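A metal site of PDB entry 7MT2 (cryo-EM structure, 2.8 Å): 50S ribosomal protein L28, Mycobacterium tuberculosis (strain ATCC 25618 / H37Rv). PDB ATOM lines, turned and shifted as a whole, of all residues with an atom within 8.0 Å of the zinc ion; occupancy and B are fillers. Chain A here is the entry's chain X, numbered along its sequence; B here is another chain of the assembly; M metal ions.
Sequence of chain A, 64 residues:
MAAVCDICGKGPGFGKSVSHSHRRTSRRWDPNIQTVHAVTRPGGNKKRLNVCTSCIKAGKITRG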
ATOM      1  N   VAL A   4     -26.371  22.653   9.804  1.00  0.00           N
ATOM      2  CA  VAL A   4     -27.742  22.279   9.495  1.00  0.00           C
ATOM      3  C   VAL A   4     -28.071  21.008  10.264  1.00  0.00           C
ATOM      4  O   VAL A   4     -27.403  19.987  10.086  1.00  0.00           O
ATOM      5  CB  VAL A   4     -27.964  22.058   7.991  1.00  0.00           C
ATOM      6  CG1 VAL A   4     -29.369  21.593   7.738  1.00  0.00           C
ATOM      7  CG2 VAL A   4     -27.709  23.328   7.221  1.00  0.00           C
ATOM      8  N   CYS A   5     -29.079  21.084  11.118  1.00  0.00           N
ATOM      9  CA  CYS A   5     -29.497  19.925  11.900  1.00  0.00           C
ATOM     10  C   CYS A   5     -30.216  18.916  11.010  1.00  0.00           C
ATOM     11  O   CYS A   5     -31.012  19.282  10.153  1.00  0.00           O
ATOM     12  CB  CYS A   5     -30.404  20.357  13.035  1.00  0.00           C
ATOM     13  SG  CYS A   5     -30.950  19.023  14.109  1.00  0.00           S
ATOM     14  N   ASP A   6     -29.920  17.640  11.223  1.00  0.00           N
ATOM     15  CA  ASP A   6     -30.449  16.566  10.404  1.00  0.00           C
ATOM     16  C   ASP A   6     -31.784  16.019  10.908  1.00  0.00           C
ATOM     17  O   ASP A   6     -32.214  14.964  10.439  1.00  0.00           O
ATOM     18  CB  ASP A   6     -29.438  15.423  10.304  1.00  0.00           C
ATOM     19  CG  ASP A   6     -28.263  15.757   9.402  1.00  0.00           C
ATOM     20  OD1 ASP A   6     -28.441  16.560   8.464  1.00  0.00           O
ATOM     21  OD2 ASP A   6     -27.166  15.208   9.622  1.00  0.00           O
ATOM     22  N   ILE A   7     -32.440  16.692  11.852  1.00  0.00           N
ATOM     23  CA  ILE A   7     -33.771  16.274  12.274  1.00  0.00           C
ATOM     24  C   ILE A   7     -34.770  17.391  12.069  1.00  0.00           C
ATOM     25  O   ILE A   7     -35.742  17.241  11.325  1.00  0.00           O
ATOM     26  CB  ILE A   7     -33.766  15.810  13.740  1.00  0.00           C
ATOM     27  CG1 ILE A   7     -32.944  14.538  13.890  1.00  0.00           C
ATOM     28  CG2 ILE A   7     -35.185  15.582  14.221  1.00  0.00           C
ATOM     29  CD1 ILE A   7     -32.816  14.120  15.291  1.00  0.00           C
ATOM     30  N   CYS A   8     -34.554  18.529  12.734  1.00  0.00           N
ATOM     31  CA  CYS A   8     -35.497  19.633  12.678  1.00  0.00           C
ATOM     32  C   CYS A   8     -35.206  20.613  11.564  1.00  0.00           C
ATOM     33  O   CYS A   8     -35.974  21.556  11.369  1.00  0.00           O
ATOM     34  CB  CYS A   8     -35.543  20.358  14.026  1.00  0.00           C
ATOM     35  SG  CYS A   8     -33.996  21.127  14.536  1.00  0.00           S
ATOM     36  N   GLY A   9     -34.124  20.416  10.817  1.00  0.00           N
ATOM     37  CA  GLY A   9     -33.819  21.260   9.679  1.00  0.00           C
ATOM     38  C   GLY A   9     -33.387  22.670  10.038  1.00  0.00           C
ATOM     39  O   GLY A   9     -33.455  23.552   9.187  1.00  0.00           O
ATOM     40  N   LYS A  10     -32.944  22.892  11.272  1.00  0.00           N
ATOM     41  CA  LYS A  10     -32.608  24.223  11.731  1.00  0.00           C
ATOM     42  C   LYS A  10     -31.269  24.650  11.161  1.00  0.00           C
ATOM     43  O   LYS A  10     -30.259  23.958  11.338  1.00  0.00           O
ATOM     44  CB  LYS A  10     -32.586  24.258  13.260  1.00  0.00           C
ATOM     45  CG  LYS A  10     -32.298  25.614  13.840  1.00  0.00           C
ATOM     46  CD  LYS A  10     -32.730  25.691  15.281  1.00  0.00           C
ATOM     47  CE  LYS A  10     -31.809  24.956  16.203  1.00  0.00           C
ATOM     48  NZ  LYS A  10     -32.230  25.189  17.608  1.00  0.00           N
ATOM     49  N   PRO A  31     -25.990  27.286  14.444  1.00  0.00           N
ATOM     50  CA  PRO A  31     -26.531  26.559  15.585  1.00  0.00           C
ATOM     51  C   PRO A  31     -25.539  25.581  16.181  1.00  0.00           C
ATOM     52  O   PRO A  31     -24.594  25.128  15.535  1.00  0.00           O
ATOM     53  CB  PRO A  31     -27.727  25.823  14.989  1.00  0.00           C
ATOM     54  CG  PRO A  31     -27.373  25.663  13.607  1.00  0.00           C
ATOM     55  CD  PRO A  31     -26.610  26.860  13.191  1.00  0.00           C
ATOM     56  N   ASN A  32     -25.795  25.240  17.442  1.00  0.00           N
ATOM     57  CA  ASN A  32     -24.927  24.395  18.242  1.00  0.00           C
ATOM     58  C   ASN A  32     -25.113  22.947  17.798  1.00  0.00           C
ATOM     59  O   ASN A  32     -25.819  22.151  18.417  1.00  0.00           O
ATOM     60  CB  ASN A  32     -25.247  24.572  19.716  1.00  0.00           C
ATOM     61  CG  ASN A  32     -24.172  24.039  20.610  1.00  0.00           C
ATOM     62  OD1 ASN A  32     -23.163  23.521  20.157  1.00  0.00           O
ATOM     63  ND2 ASN A  32     -24.374  24.189  21.914  1.00  0.00           N
ATOM     64  N   ILE A  33     -24.457  22.596  16.689  1.00  0.00           N
ATOM     65  CA  ILE A  33     -24.572  21.259  16.109  1.00  0.00           C
ATOM     66  C   ILE A  33     -23.541  20.360  16.777  1.00  0.00           C
ATOM     67  O   ILE A  33     -22.343  20.646  16.732  1.00  0.00           O
ATOM     68  CB  ILE A  33     -24.362  21.289  14.593  1.00  0.00           C
ATOM     69  CG1 ILE A  33     -25.373  22.223  13.933  1.00  0.00           C
ATOM     70  CG2 ILE A  33     -24.475  19.907  14.022  1.00  0.00           C
ATOM     71  CD1 ILE A  33     -26.800  21.830  14.168  1.00  0.00           C
ATOM     72  N   ASN A  50     -25.810  14.589  12.602  1.00  0.00           N
ATOM     73  CA  ASN A  50     -25.501  15.941  13.061  1.00  0.00           C
ATOM     74  C   ASN A  50     -26.785  16.548  13.604  1.00  0.00           C
ATOM     75  O   ASN A  50     -27.683  16.896  12.827  1.00  0.00           O
ATOM     76  CB  ASN A  50     -24.959  16.802  11.923  1.00  0.00           C
ATOM     77  CG  ASN A  50     -23.594  16.369  11.463  1.00  0.00           C
ATOM     78  OD1 ASN A  50     -22.742  15.990  12.259  1.00  0.00           O
ATOM     79  ND2 ASN A  50     -23.367  16.445  10.156  1.00  0.00           N
ATOM     80  N   VAL A  51     -26.883  16.671  14.916  1.00  0.00           N
ATOM     81  CA  VAL A  51     -28.083  17.200  15.551  1.00  0.00           C
ATOM     82  C   VAL A  51     -27.695  18.412  16.395  1.00  0.00           C
ATOM     83  O   VAL A  51     -26.530  18.611  16.744  1.00  0.00           O
ATOM     84  CB  VAL A  51     -28.792  16.154  16.423  1.00  0.00           C
ATOM     85  CG1 VAL A  51     -29.204  14.976  15.595  1.00  0.00           C
ATOM     86  CG2 VAL A  51     -27.889  15.702  17.517  1.00  0.00           C
ATOM     87  N   CYS A  52     -28.689  19.225  16.710  1.00  0.00           N
ATOM     88  CA  CYS A  52     -28.467  20.402  17.532  1.00  0.00           C
ATOM     89  C   CYS A  52     -28.720  20.057  18.993  1.00  0.00           C
ATOM     90  O   CYS A  52     -29.310  19.029  19.321  1.00  0.00           O
ATOM     91  CB  CYS A  52     -29.366  21.551  17.091  1.00  0.00           C
ATOM     92  SG  CYS A  52     -31.122  21.259  17.347  1.00  0.00           S
ATOM     93  N   THR A  53     -28.258  20.939  19.880  1.00  0.00           N
ATOM     94  CA  THR A  53     -28.376  20.655  21.307  1.00  0.00           C
ATOM     95  C   THR A  53     -29.794  20.820  21.819  1.00  0.00           C
ATOM     96  O   THR A  53     -30.124  20.245  22.861  1.00  0.00           O
ATOM     97  CB  THR A  53     -27.440  21.549  22.105  1.00  0.00           C
ATOM     98  OG1 THR A  53     -27.732  22.925  21.805  1.00  0.00           O
ATOM     99  CG2 THR A  53     -26.026  21.247  21.761  1.00  0.00           C
ATOM    100  N   SER A  54     -30.635  21.566  21.116  1.00  0.00           N
ATOM    101  CA  SER A  54     -32.025  21.661  21.521  1.00  0.00           C
ATOM    102  C   SER A  54     -32.816  20.401  21.200  1.00  0.00           C
ATOM    103  O   SER A  54     -33.909  20.221  21.730  1.00  0.00           O
ATOM    104  CB  SER A  54     -32.687  22.862  20.870  1.00  0.00           C
ATOM    105  OG  SER A  54     -32.754  22.703  19.471  1.00  0.00           O
ATOM    106  N   CYS A  55     -32.292  19.527  20.344  1.00  0.00           N
ATOM    107  CA  CYS A  55     -32.921  18.242  20.052  1.00  0.00           C
ATOM    108  C   CYS A  55     -32.259  17.079  20.766  1.00  0.00           C
ATOM    109  O   CYS A  55     -32.731  15.954  20.649  1.00  0.00           O
ATOM    110  CB  CYS A  55     -32.941  17.981  18.551  1.00  0.00           C
ATOM    111  SG  CYS A  55     -34.011  19.092  17.642  1.00  0.00           S
ATOM    112  N   ILE A  56     -31.164  17.323  21.486  1.00  0.00           N
ATOM    113  CA  ILE A  56     -30.664  16.331  22.427  1.00  0.00           C
ATOM    114  C   ILE A  56     -31.292  16.569  23.789  1.00  0.00           C
ATOM    115  O   ILE A  56     -31.479  15.627  24.561  1.00  0.00           O
ATOM    116  CB  ILE A  56     -29.135  16.377  22.494  1.00  0.00           C
ATOM    117  CG1 ILE A  56     -28.541  16.265  21.102  1.00  0.00           C
ATOM    118  CG2 ILE A  56     -28.571  15.219  23.284  1.00  0.00           C
ATOM    119  CD1 ILE A  56     -27.067  16.542  21.065  1.00  0.00           C
ATOM    120  N   LYS A  60     -35.512  13.529  21.101  1.00  0.00           N
ATOM    121  CA  LYS A  60     -35.558  13.283  19.670  1.00  0.00           C
ATOM    122  C   LYS A  60     -34.653  12.132  19.235  1.00  0.00           C
ATOM    123  O   LYS A  60     -34.903  11.536  18.187  1.00  0.00           O
ATOM    124  CB  LYS A  60     -35.193  14.543  18.896  1.00  0.00           C
ATOM    125  CG  LYS A  60     -36.074  15.772  19.151  1.00  0.00           C
ATOM    126  CD  LYS A  60     -37.434  15.724  18.456  1.00  0.00           C
ATOM    127  CE  LYS A  60     -38.569  15.368  19.417  1.00  0.00           C
ATOM    128  NZ  LYS A  60     -39.903  15.421  18.761  1.00  0.00           N
ATOM    129  P     U B 486     -29.470  27.199  18.340  1.00  0.00           P
ATOM    130  OP1   U B 486     -28.943  25.850  18.081  1.00  0.00           O
ATOM    131  OP2   U B 486     -30.919  27.377  18.542  1.00  0.00           O
ATOM    132  O5'   U B 486     -28.713  27.757  19.611  1.00  0.00           O
ATOM    133  C5'   U B 486     -27.294  27.839  19.635  1.00  0.00           C
ATOM    134  C4'   U B 486     -26.825  28.562  20.867  1.00  0.00           C
ATOM    135  O4'   U B 486     -27.219  29.949  20.795  1.00  0.00           O
ATOM    136  C3'   U B 486     -27.403  28.074  22.181  1.00  0.00           C
ATOM    137  O3'   U B 486     -26.780  26.926  22.698  1.00  0.00           O
ATOM    138  C2'   U B 486     -27.257  29.294  23.071  1.00  0.00           C
ATOM    139  O2'   U B 486     -25.925  29.409  23.535  1.00  0.00           O
ATOM    140  C1'   U B 486     -27.510  30.429  22.090  1.00  0.00           C
ATOM    141  N1    U B 486     -28.909  30.908  22.122  1.00  0.00           N
ATOM    142  C2    U B 486     -29.288  31.745  23.140  1.00  0.00           C
ATOM    143  O2    U B 486     -28.535  32.133  24.014  1.00  0.00           O
ATOM    144  N3    U B 486     -30.591  32.150  23.108  1.00  0.00           N
ATOM    145  C4    U B 486     -31.543  31.815  22.183  1.00  0.00           C
ATOM    146  O4    U B 486     -32.681  32.266  22.298  1.00  0.00           O
ATOM    147  C5    U B 486     -31.091  30.950  21.163  1.00  0.00           C
ATOM    148  C6    U B 486     -29.825  30.543  21.169  1.00  0.00           C
HETATM  149 ZN    ZN M   1     -32.446  19.784  15.883  1.00  0.00          ZN
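The nearest printed residue that does not touch the zinc ion is Ser 54 (4.6 Å).
The side-chain sulfur (SG) of Cys 5 sits close to the backbone NH (N) of Ile 7, 3.6 Å away.
The backbone NH (N) of Cys 5 is in hydrogen-bond range of the backbone carbonyl oxygen (O) of Lys 10 (3.1 Å).
OG of Ser 54 sits close to SG of Cys 52.
The zinc ion is bound by the side-chain sulfur (SG) of Cys 5 (2.4 Å), the side-chain sulfur (SG) of Cys 8 (2.5 Å), the side-chain sulfur (SG) of Cys 55 (2.5 Å) and the side-chain sulfur (SG) of Cys 52 (2.5 Å).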
